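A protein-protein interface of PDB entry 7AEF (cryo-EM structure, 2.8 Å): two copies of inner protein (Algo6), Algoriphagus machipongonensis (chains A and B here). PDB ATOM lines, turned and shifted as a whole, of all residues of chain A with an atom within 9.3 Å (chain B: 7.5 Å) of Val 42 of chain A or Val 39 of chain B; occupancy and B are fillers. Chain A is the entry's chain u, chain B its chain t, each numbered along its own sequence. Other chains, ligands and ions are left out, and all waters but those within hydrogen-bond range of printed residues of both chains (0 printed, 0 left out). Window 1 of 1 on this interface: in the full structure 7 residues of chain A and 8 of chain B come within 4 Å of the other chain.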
ATOM      1  N   GLU A   7      29.020   9.524  -6.335  1.00  0.00           N
ATOM      2  CA  GLU A   7      29.544   8.705  -7.416  1.00  0.00           C
ATOM      3  C   GLU A   7      30.254   9.503  -8.498  1.00  0.00           C
ATOM      4  O   GLU A   7      30.528   8.954  -9.568  1.00  0.00           O
ATOM      5  CB  GLU A   7      28.404   7.895  -8.030  1.00  0.00           C
ATOM      6  CG  GLU A   7      27.618   7.113  -7.000  1.00  0.00           C
ATOM      7  CD  GLU A   7      26.323   6.567  -7.543  1.00  0.00           C
ATOM      8  OE1 GLU A   7      25.941   6.957  -8.663  1.00  0.00           O
ATOM      9  OE2 GLU A   7      25.687   5.746  -6.852  1.00  0.00           O
ATOM     10  N   VAL A  35      34.362   8.213 -20.704  1.00  0.00           N
ATOM     11  CA  VAL A  35      34.659   7.523 -19.451  1.00  0.00           C
ATOM     12  C   VAL A  35      33.560   7.786 -18.430  1.00  0.00           C
ATOM     13  O   VAL A  35      33.206   6.905 -17.640  1.00  0.00           O
ATOM     14  CB  VAL A  35      36.053   7.941 -18.932  1.00  0.00           C
ATOM     15  CG1 VAL A  35      36.408   7.242 -17.633  1.00  0.00           C
ATOM     16  CG2 VAL A  35      37.115   7.613 -19.960  1.00  0.00           C
ATOM     17  N   ALA A  36      32.954   8.973 -18.481  1.00  0.00           N
ATOM     18  CA  ALA A  36      31.903   9.311 -17.528  1.00  0.00           C
ATOM     19  C   ALA A  36      30.617   8.539 -17.801  1.00  0.00           C
ATOM     20  O   ALA A  36      29.828   8.296 -16.883  1.00  0.00           O
ATOM     21  CB  ALA A  36      31.641  10.813 -17.555  1.00  0.00           C
ATOM     22  N   GLN A  37      30.387   8.142 -19.055  1.00  0.00           N
ATOM     23  CA  GLN A  37      29.221   7.319 -19.371  1.00  0.00           C
ATOM     24  C   GLN A  37      29.405   5.878 -18.915  1.00  0.00           C
ATOM     25  O   GLN A  37      28.428   5.195 -18.599  1.00  0.00           O
ATOM     26  CB  GLN A  37      28.939   7.342 -20.867  1.00  0.00           C
ATOM     27  CG  GLN A  37      28.125   8.509 -21.349  1.00  0.00           C
ATOM     28  CD  GLN A  37      27.823   8.402 -22.826  1.00  0.00           C
ATOM     29  OE1 GLN A  37      28.304   7.494 -23.496  1.00  0.00           O
ATOM     30  NE2 GLN A  37      26.989   9.300 -23.329  1.00  0.00           N
ATOM     31  N   CYS A  38      30.647   5.394 -18.893  1.00  0.00           N
ATOM     32  CA  CYS A  38      30.892   4.011 -18.510  1.00  0.00           C
ATOM     33  C   CYS A  38      30.767   3.820 -17.004  1.00  0.00           C
ATOM     34  O   CYS A  38      30.397   2.737 -16.545  1.00  0.00           O
ATOM     35  CB  CYS A  38      32.270   3.576 -19.001  1.00  0.00           C
ATOM     36  SG  CYS A  38      32.370   3.317 -20.786  1.00  0.00           S
ATOM     37  N   VAL A  39      31.061   4.856 -16.220  1.00  0.00           N
ATOM     38  CA  VAL A  39      30.897   4.757 -14.770  1.00  0.00           C
ATOM     39  C   VAL A  39      29.420   4.813 -14.397  1.00  0.00           C
ATOM     40  O   VAL A  39      28.995   4.229 -13.395  1.00  0.00           O
ATOM     41  CB  VAL A  39      31.725   5.854 -14.064  1.00  0.00           C
ATOM     42  CG1 VAL A  39      31.748   5.661 -12.560  1.00  0.00           C
ATOM     43  CG2 VAL A  39      33.148   5.840 -14.559  1.00  0.00           C
ATOM     44  N   GLU A  40      28.653   5.529 -15.170  1.00  0.00           N
ATOM     45  CA  GLU A  40      27.246   5.613 -14.945  1.00  0.00           C
ATOM     46  C   GLU A  40      26.495   4.292 -15.175  1.00  0.00           C
ATOM     47  O   GLU A  40      25.641   3.969 -14.392  1.00  0.00           O
ATOM     48  CB  GLU A  40      26.716   6.724 -15.819  1.00  0.00           C
ATOM     49  CG  GLU A  40      25.437   7.370 -15.362  1.00  0.00           C
ATOM     50  CD  GLU A  40      24.866   8.228 -16.454  1.00  0.00           C
ATOM     51  OE1 GLU A  40      23.691   8.613 -16.361  1.00  0.00           O
ATOM     52  OE2 GLU A  40      25.599   8.508 -17.421  1.00  0.00           O
ATOM     53  N   GLN A  41      26.858   3.506 -16.195  1.00  0.00           N
ATOM     54  CA  GLN A  41      26.141   2.282 -16.542  1.00  0.00           C
ATOM     55  C   GLN A  41      26.584   1.103 -15.686  1.00  0.00           C
ATOM     56  O   GLN A  41      25.821   0.147 -15.506  1.00  0.00           O
ATOM     57  CB  GLN A  41      26.331   1.963 -18.019  1.00  0.00           C
ATOM     58  CG  GLN A  41      25.903   3.083 -18.935  1.00  0.00           C
ATOM     59  CD  GLN A  41      25.300   2.581 -20.221  1.00  0.00           C
ATOM     60  OE1 GLN A  41      24.729   1.498 -20.267  1.00  0.00           O
ATOM     61  NE2 GLN A  41      25.430   3.365 -21.278  1.00  0.00           N
ATOM     62  N   VAL A  42      27.814   1.136 -15.166  1.00  0.00           N
ATOM     63  CA  VAL A  42      28.270   0.075 -14.272  1.00  0.00           C
ATOM     64  C   VAL A  42      27.526   0.152 -12.943  1.00  0.00           C
ATOM     65  O   VAL A  42      27.039  -0.861 -12.427  1.00  0.00           O
ATOM     66  CB  VAL A  42      29.799   0.151 -14.079  1.00  0.00           C
ATOM     67  CG1 VAL A  42      30.243  -0.661 -12.882  1.00  0.00           C
ATOM     68  CG2 VAL A  42      30.519  -0.335 -15.310  1.00  0.00           C
ATOM     69  N   LEU A  43      27.392   1.359 -12.391  1.00  0.00           N
ATOM     70  CA  LEU A  43      26.785   1.511 -11.075  1.00  0.00           C
ATOM     71  C   LEU A  43      25.276   1.317 -11.111  1.00  0.00           C
ATOM     72  O   LEU A  43      24.666   1.077 -10.067  1.00  0.00           O
ATOM     73  CB  LEU A  43      27.132   2.883 -10.499  1.00  0.00           C
ATOM     74  CG  LEU A  43      28.619   3.175 -10.287  1.00  0.00           C
ATOM     75  CD1 LEU A  43      28.804   4.567  -9.732  1.00  0.00           C
ATOM     76  CD2 LEU A  43      29.273   2.144  -9.387  1.00  0.00           C
ATOM     77  N   ASP A  44      24.662   1.415 -12.288  1.00  0.00           N
ATOM     78  CA  ASP A  44      23.248   1.072 -12.414  1.00  0.00           C
ATOM     79  C   ASP A  44      23.044  -0.436 -12.460  1.00  0.00           C
ATOM     80  O   ASP A  44      22.013  -0.940 -12.008  1.00  0.00           O
ATOM     81  CB  ASP A  44      22.653   1.721 -13.657  1.00  0.00           C
ATOM     82  CG  ASP A  44      22.537   3.219 -13.529  1.00  0.00           C
ATOM     83  OD1 ASP A  44      22.456   3.719 -12.386  1.00  0.00           O
ATOM     84  OD2 ASP A  44      22.500   3.905 -14.575  1.00  0.00           O
ATOM     85  N   VAL A  45      24.009  -1.165 -13.021  1.00  0.00           N
ATOM     86  CA  VAL A  45      23.938  -2.620 -13.054  1.00  0.00           C
ATOM     87  C   VAL A  45      24.137  -3.194 -11.655  1.00  0.00           C
ATOM     88  O   VAL A  45      23.467  -4.156 -11.263  1.00  0.00           O
ATOM     89  CB  VAL A  45      24.963  -3.162 -14.074  1.00  0.00           C
ATOM     90  CG1 VAL A  45      25.240  -4.644 -13.892  1.00  0.00           C
ATOM     91  CG2 VAL A  45      24.483  -2.904 -15.485  1.00  0.00           C
ATOM     92  N   LEU A  46      25.015  -2.579 -10.858  1.00  0.00           N
ATOM     93  CA  LEU A  46      25.271  -3.064  -9.505  1.00  0.00           C
ATOM     94  C   LEU A  46      24.088  -2.807  -8.585  1.00  0.00           C
ATOM     95  O   LEU A  46      23.848  -3.569  -7.644  1.00  0.00           O
ATOM     96  CB  LEU A  46      26.525  -2.408  -8.937  1.00  0.00           C
ATOM     97  CG  LEU A  46      27.855  -2.764  -9.595  1.00  0.00           C
ATOM     98  CD1 LEU A  46      28.950  -1.882  -9.053  1.00  0.00           C
ATOM     99  CD2 LEU A  46      28.181  -4.217  -9.369  1.00  0.00           C
ATOM    100  N   LYS A  47      23.335  -1.740  -8.841  1.00  0.00           N
ATOM    101  CA  LYS A  47      22.184  -1.420  -7.999  1.00  0.00           C
ATOM    102  C   LYS A  47      21.001  -2.324  -8.312  1.00  0.00           C
ATOM    103  O   LYS A  47      20.205  -2.643  -7.421  1.00  0.00           O
ATOM    104  CB  LYS A  47      21.804   0.044  -8.188  1.00  0.00           C
ATOM    105  CG  LYS A  47      20.871   0.584  -7.131  1.00  0.00           C
ATOM    106  CD  LYS A  47      20.414   1.989  -7.458  1.00  0.00           C
ATOM    107  CE  LYS A  47      19.242   1.980  -8.426  1.00  0.00           C
ATOM    108  NZ  LYS A  47      17.993   1.479  -7.787  1.00  0.00           N
ATOM    109  N   SER A  48      20.868  -2.751  -9.571  1.00  0.00           N
ATOM    110  CA  SER A  48      19.709  -3.545  -9.966  1.00  0.00           C
ATOM    111  C   SER A  48      19.817  -4.980  -9.476  1.00  0.00           C
ATOM    112  O   SER A  48      18.814  -5.694  -9.410  1.00  0.00           O
ATOM    113  CB  SER A  48      19.551  -3.517 -11.481  1.00  0.00           C
ATOM    114  OG  SER A  48      19.239  -2.218 -11.936  1.00  0.00           O
ATOM    115  N   GLN A  49      21.027  -5.424  -9.130  1.00  0.00           N
ATOM    116  CA  GLN A  49      21.216  -6.809  -8.719  1.00  0.00           C
ATOM    117  C   GLN A  49      20.745  -7.039  -7.290  1.00  0.00           C
ATOM    118  O   GLN A  49      20.499  -8.181  -6.889  1.00  0.00           O
ATOM    119  CB  GLN A  49      22.678  -7.202  -8.869  1.00  0.00           C
ATOM    120  CG  GLN A  49      23.121  -7.364 -10.300  1.00  0.00           C
ATOM    121  CD  GLN A  49      24.613  -7.516 -10.424  1.00  0.00           C
ATOM    122  OE1 GLN A  49      25.365  -7.043  -9.577  1.00  0.00           O
ATOM    123  NE2 GLN A  49      25.057  -8.182 -11.479  1.00  0.00           N
ATOM    124  N   LYS A  50      20.620  -5.972  -6.502  1.00  0.00           N
ATOM    125  CA  LYS A  50      20.141  -6.118  -5.136  1.00  0.00           C
ATOM    126  C   LYS A  50      18.626  -6.040  -5.031  1.00  0.00           C
ATOM    127  O   LYS A  50      18.089  -6.114  -3.922  1.00  0.00           O
ATOM    128  CB  LYS A  50      20.786  -5.064  -4.244  1.00  0.00           C
ATOM    129  CG  LYS A  50      22.241  -5.333  -3.960  1.00  0.00           C
ATOM    130  CD  LYS A  50      22.790  -4.361  -2.946  1.00  0.00           C
ATOM    131  CE  LYS A  50      23.007  -2.992  -3.562  1.00  0.00           C
ATOM    132  NZ  LYS A  50      24.128  -3.000  -4.538  1.00  0.00           N
ATOM    133  N   PRO B   2      29.017 -11.962 -20.789  1.00  0.00           N
ATOM    134  CA  PRO B   2      28.528 -12.538 -19.532  1.00  0.00           C
ATOM    135  C   PRO B   2      27.702 -13.796 -19.748  1.00  0.00           C
ATOM    136  O   PRO B   2      27.070 -13.933 -20.788  1.00  0.00           O
ATOM    137  CB  PRO B   2      27.668 -11.414 -18.945  1.00  0.00           C
ATOM    138  CG  PRO B   2      27.356 -10.520 -20.089  1.00  0.00           C
ATOM    139  CD  PRO B   2      28.535 -10.586 -20.986  1.00  0.00           C
ATOM    140  N   GLU B   7      23.187  -8.865 -15.958  1.00  0.00           N
ATOM    141  CA  GLU B   7      24.186  -7.819 -16.096  1.00  0.00           C
ATOM    142  C   GLU B   7      24.075  -7.035 -17.395  1.00  0.00           C
ATOM    143  O   GLU B   7      25.000  -6.290 -17.728  1.00  0.00           O
ATOM    144  CB  GLU B   7      25.578  -8.434 -15.978  1.00  0.00           C
ATOM    145  CG  GLU B   7      25.744  -9.273 -14.730  1.00  0.00           C
ATOM    146  CD  GLU B   7      26.988 -10.124 -14.757  1.00  0.00           C
ATOM    147  OE1 GLU B   7      27.622 -10.209 -15.826  1.00  0.00           O
ATOM    148  OE2 GLU B   7      27.334 -10.707 -13.709  1.00  0.00           O
ATOM    149  N   LEU B   8      22.980  -7.173 -18.131  1.00  0.00           N
ATOM    150  CA  LEU B   8      22.801  -6.410 -19.356  1.00  0.00           C
ATOM    151  C   LEU B   8      22.070  -5.100 -19.072  1.00  0.00           C
ATOM    152  O   LEU B   8      21.218  -5.015 -18.187  1.00  0.00           O
ATOM    153  CB  LEU B   8      22.037  -7.242 -20.391  1.00  0.00           C
ATOM    154  CG  LEU B   8      22.617  -8.625 -20.715  1.00  0.00           C
ATOM    155  CD1 LEU B   8      21.624  -9.490 -21.457  1.00  0.00           C
ATOM    156  CD2 LEU B   8      23.912  -8.519 -21.504  1.00  0.00           C
ATOM    157  N   HIS B   9      22.409  -4.069 -19.843  1.00  0.00           N
ATOM    158  CA  HIS B   9      21.833  -2.741 -19.696  1.00  0.00           C
ATOM    159  C   HIS B   9      20.997  -2.422 -20.928  1.00  0.00           C
ATOM    160  O   HIS B   9      21.249  -2.947 -22.013  1.00  0.00           O
ATOM    161  CB  HIS B   9      22.929  -1.681 -19.509  1.00  0.00           C
ATOM    162  CG  HIS B   9      22.483  -0.463 -18.764  1.00  0.00           C
ATOM    163  ND1 HIS B   9      22.190  -0.480 -17.417  1.00  0.00           N
ATOM    164  CD2 HIS B   9      22.297   0.814 -19.172  1.00  0.00           C
ATOM    165  CE1 HIS B   9      21.833   0.732 -17.030  1.00  0.00           C
ATOM    166  NE2 HIS B   9      21.889   1.536 -18.076  1.00  0.00           N
ATOM    167  N   LEU B  34      31.520   0.188 -27.390  1.00  0.00           N
ATOM    168  CA  LEU B  34      32.647   0.453 -26.502  1.00  0.00           C
ATOM    169  C   LEU B  34      32.214   0.461 -25.043  1.00  0.00           C
ATOM    170  O   LEU B  34      32.948  -0.015 -24.173  1.00  0.00           O
ATOM    171  CB  LEU B  34      33.304   1.781 -26.865  1.00  0.00           C
ATOM    172  CG  LEU B  34      34.404   1.735 -27.922  1.00  0.00           C
ATOM    173  CD1 LEU B  34      34.589   3.108 -28.535  1.00  0.00           C
ATOM    174  CD2 LEU B  34      35.701   1.235 -27.310  1.00  0.00           C
ATOM    175  N   VAL B  35      31.036   1.020 -24.756  1.00  0.00           N
ATOM    176  CA  VAL B  35      30.543   1.066 -23.381  1.00  0.00           C
ATOM    177  C   VAL B  35      30.180  -0.334 -22.904  1.00  0.00           C
ATOM    178  O   VAL B  35      30.382  -0.677 -21.735  1.00  0.00           O
ATOM    179  CB  VAL B  35      29.355   2.047 -23.273  1.00  0.00           C
ATOM    180  CG1 VAL B  35      28.815   2.132 -21.857  1.00  0.00           C
ATOM    181  CG2 VAL B  35      29.780   3.434 -23.708  1.00  0.00           C
ATOM    182  N   ALA B  36      29.711  -1.185 -23.816  1.00  0.00           N
ATOM    183  CA  ALA B  36      29.323  -2.540 -23.440  1.00  0.00           C
ATOM    184  C   ALA B  36      30.533  -3.410 -23.118  1.00  0.00           C
ATOM    185  O   ALA B  36      30.428  -4.359 -22.336  1.00  0.00           O
ATOM    186  CB  ALA B  36      28.492  -3.171 -24.552  1.00  0.00           C
ATOM    187  N   GLN B  37      31.691  -3.101 -23.706  1.00  0.00           N
ATOM    188  CA  GLN B  37      32.912  -3.834 -23.372  1.00  0.00           C
ATOM    189  C   GLN B  37      33.460  -3.431 -22.011  1.00  0.00           C
ATOM    190  O   GLN B  37      34.103  -4.237 -21.335  1.00  0.00           O
ATOM    191  CB  GLN B  37      33.981  -3.608 -24.433  1.00  0.00           C
ATOM    192  CG  GLN B  37      33.889  -4.501 -25.637  1.00  0.00           C
ATOM    193  CD  GLN B  37      35.035  -4.263 -26.592  1.00  0.00           C
ATOM    194  OE1 GLN B  37      35.845  -3.365 -26.383  1.00  0.00           O
ATOM    195  NE2 GLN B  37      35.137  -5.095 -27.617  1.00  0.00           N
ATOM    196  N   CYS B  38      33.231  -2.183 -21.603  1.00  0.00           N
ATOM    197  CA  CYS B  38      33.764  -1.716 -20.330  1.00  0.00           C
ATOM    198  C   CYS B  38      32.968  -2.270 -19.155  1.00  0.00           C
ATOM    199  O   CYS B  38      33.520  -2.464 -18.070  1.00  0.00           O
ATOM    200  CB  CYS B  38      33.778  -0.190 -20.305  1.00  0.00           C
ATOM    201  SG  CYS B  38      35.050   0.553 -21.350  1.00  0.00           S
ATOM    202  N   VAL B  39      31.678  -2.536 -19.351  1.00  0.00           N
ATOM    203  CA  VAL B  39      30.877  -3.132 -18.283  1.00  0.00           C
ATOM    204  C   VAL B  39      31.222  -4.608 -18.119  1.00  0.00           C
ATOM    205  O   VAL B  39      31.126  -5.163 -17.020  1.00  0.00           O
ATOM    206  CB  VAL B  39      29.371  -2.907 -18.557  1.00  0.00           C
ATOM    207  CG1 VAL B  39      28.516  -3.324 -17.376  1.00  0.00           C
ATOM    208  CG2 VAL B  39      29.101  -1.451 -18.838  1.00  0.00           C
ATOM    209  N   GLU B  40      31.586  -5.243 -19.197  1.00  0.00           N
ATOM    210  CA  GLU B  40      31.980  -6.613 -19.153  1.00  0.00           C
ATOM    211  C   GLU B  40      33.286  -6.865 -18.383  1.00  0.00           C
ATOM    212  O   GLU B  40      33.347  -7.808 -17.641  1.00  0.00           O
ATOM    213  CB  GLU B  40      32.056  -7.106 -20.577  1.00  0.00           C
ATOM    214  CG  GLU B  40      31.888  -8.588 -20.774  1.00  0.00           C
ATOM    215  CD  GLU B  40      32.285  -8.978 -22.168  1.00  0.00           C
ATOM    216  OE1 GLU B  40      32.473 -10.176 -22.424  1.00  0.00           O
ATOM    217  OE2 GLU B  40      32.420  -8.072 -23.012  1.00  0.00           O
ATOM    218  N   GLN B  41      34.292  -5.992 -18.509  1.00  0.00           N
ATOM    219  CA  GLN B  41      35.600  -6.201 -17.891  1.00  0.00           C
ATOM    220  C   GLN B  41      35.613  -5.763 -16.433  1.00  0.00           C
ATOM    221  O   GLN B  41      36.429  -6.258 -15.647  1.00  0.00           O
ATOM    222  CB  GLN B  41      36.676  -5.461 -18.676  1.00  0.00           C
ATOM    223  CG  GLN B  41      36.730  -5.849 -20.133  1.00  0.00           C
ATOM    224  CD  GLN B  41      38.134  -5.842 -20.681  1.00  0.00           C
ATOM    225  OE1 GLN B  41      39.095  -6.054 -19.951  1.00  0.00           O
ATOM    226  NE2 GLN B  41      38.260  -5.588 -21.974  1.00  0.00           N
ATOM    227  N   VAL B  42      34.739  -4.827 -16.055  1.00  0.00           N
ATOM    228  CA  VAL B  42      34.649  -4.422 -14.654  1.00  0.00           C
ATOM    229  C   VAL B  42      34.056  -5.550 -13.817  1.00  0.00           C
ATOM    230  O   VAL B  42      34.575  -5.888 -12.748  1.00  0.00           O
ATOM    231  CB  VAL B  42      33.831  -3.119 -14.520  1.00  0.00           C
ATOM    232  CG1 VAL B  42      33.392  -2.889 -13.090  1.00  0.00           C
ATOM    233  CG2 VAL B  42      34.633  -1.934 -14.995  1.00  0.00           C
ATOM    234  N   LEU B  43      32.986  -6.175 -14.311  1.00  0.00           N
ATOM    235  CA  LEU B  43      32.296  -7.196 -13.533  1.00  0.00           C
ATOM    236  C   LEU B  43      33.079  -8.500 -13.471  1.00  0.00           C
ATOM    237  O   LEU B  43      32.816  -9.331 -12.598  1.00  0.00           O
ATOM    238  CB  LEU B  43      30.904  -7.437 -14.113  1.00  0.00           C
ATOM    239  CG  LEU B  43      29.955  -6.238 -14.124  1.00  0.00           C
ATOM    240  CD1 LEU B  43      28.631  -6.624 -14.738  1.00  0.00           C
ATOM    241  CD2 LEU B  43      29.758  -5.662 -12.733  1.00  0.00           C
ATOM    242  N   ASP B  44      34.034  -8.699 -14.378  1.00  0.00           N
ATOM    243  CA  ASP B  44      34.929  -9.847 -14.269  1.00  0.00           C
ATOM    244  C   ASP B  44      36.006  -9.612 -13.220  1.00  0.00           C
ATOM    245  O   ASP B  44      36.472 -10.560 -12.579  1.00  0.00           O
ATOM    246  CB  ASP B  44      35.567 -10.154 -15.618  1.00  0.00           C
ATOM    247  CG  ASP B  44      34.577 -10.703 -16.615  1.00  0.00           C
ATOM    248  OD1 ASP B  44      33.556 -11.284 -16.188  1.00  0.00           O
ATOM    249  OD2 ASP B  44      34.828 -10.578 -17.834  1.00  0.00           O
ATOM    250  N   VAL B  45      36.427  -8.360 -13.046  1.00  0.00           N
ATOM    251  CA  VAL B  45      37.407  -8.025 -12.021  1.00  0.00           C
ATOM    252  C   VAL B  45      36.787  -8.147 -10.632  1.00  0.00           C
ATOM    253  O   VAL B  45      37.432  -8.623  -9.691  1.00  0.00           O
ATOM    254  CB  VAL B  45      37.979  -6.616 -12.298  1.00  0.00           C
ATOM    255  CG1 VAL B  45      38.692  -6.027 -11.094  1.00  0.00           C
ATOM    256  CG2 VAL B  45      38.925  -6.660 -13.478  1.00  0.00           C
ATOM    257  N   LEU B  46      35.512  -7.776 -10.495  1.00  0.00           N
ATOM    258  CA  LEU B  46      34.842  -7.857  -9.201  1.00  0.00           C
ATOM    259  C   LEU B  46      34.583  -9.298  -8.792  1.00  0.00           C
ATOM    260  O   LEU B  46      34.564  -9.617  -7.600  1.00  0.00           O
ATOM    261  CB  LEU B  46      33.529  -7.080  -9.236  1.00  0.00           C
ATOM    262  CG  LEU B  46      33.621  -5.565  -9.387  1.00  0.00           C
ATOM    263  CD1 LEU B  46      32.247  -4.986  -9.609  1.00  0.00           C
ATOM    264  CD2 LEU B  46      34.264  -4.953  -8.170  1.00  0.00           C
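Of chain B, only Val 39 and Val 42 come within 4 Å of Val 42 of chain A. Val 39 of chain B touches one residue of chain A. Cys 38 of chain B touches one residue of chain A. Of the printed residues of chain B, Cys 38 of chain A touches Val 35 and Cys 38. Printed residues of chain B within 4 Å of Leu 46 of chain A: Leu 43 (3.99 Å). Of the printed residues of chain A, Leu 43 of chain B touches Leu 46. Of the printed residues of chain B, Gln 49 of chain A touches Glu 7.
Cys 38 of chain A touches its own counterpart, Cys 38 of chain B. Val 42 of chain A touches Val 39 of chain B, but with the chains exchanged Val 39 of chain A does not touch Val 42 of chain B (7.7 Å). Val 42 of chain B touches its own counterpart, Val 42 of chain A. Leu 46 of chain A touches Leu 43 of chain B, but with the chains exchanged Leu 43 of chain A does not touch Leu 46 of chain B (7.7 Å). 13 positions are printed for both chains. Of the 10 pairs that touch across the chains among the printed residues, 2 have their exchanged pair printed and touching as well.
Among the printed residues, pairs that only touch across the chains: Gln 41 of chain A with His 9 of chain B (2.8 Å), Gln 49 of chain A with Glu 7 of chain B (3.5 Å), Asp 44 of chain A with His 9 of chain B (3.6 Å), Gln 41 of chain A with Val 35 of chain B (3.6 Å), Cys 38 of chain A with Cys 38 of chain B (3.8 Å), Val 45 of chain A with His 9 of chain B (3.9 Å), Val 42 of chain A with Val 42 of chain B (3.9 Å), Cys 38 of chain A with Val 35 of chain B (3.9 Å), Val 42 of chain A with Val 39 of chain B (3.96 Å) and Leu 46 of chain A with Leu 43 of chain B (3.99 Å).
Printed residues of chain B that touch a printed residue of chain A: Glu 7, His 9, Val 35, Cys 38, Val 39, Val 42 and Leu 43. Hydrophobic or aromatic side chains of chain B that line the printed part of chain A: His 9, Val 35, Val 39, Val 42 and Leu 43. Hydrophobic or aromatic side chains of chain A within 4 Å of the printed part of chain B: Val 42, Val 45 and Leu 46. Among the printed residues, 10 pairs touch across the chains. Among the printed residues, no Asp or Glu carboxylate lies within 4 Å of a Lys or Arg side-chain nitrogen of the other chain.
The side-chain amino group (NZ) of Lys 50 of chain A lies within hydrogen-bond range of the backbone carbonyl oxygen (O) of Leu 46 of chain A. O of Asp 44 of chain A is in hydrogen-bond range of OG of Ser 48 of chain A (3.1 Å). The backbone carbonyl oxygen (O) of Leu 34 of chain B is in hydrogen-bond range of the side-chain sulfur (SG) of Cys 38 of chain B, 3.6 Å away.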
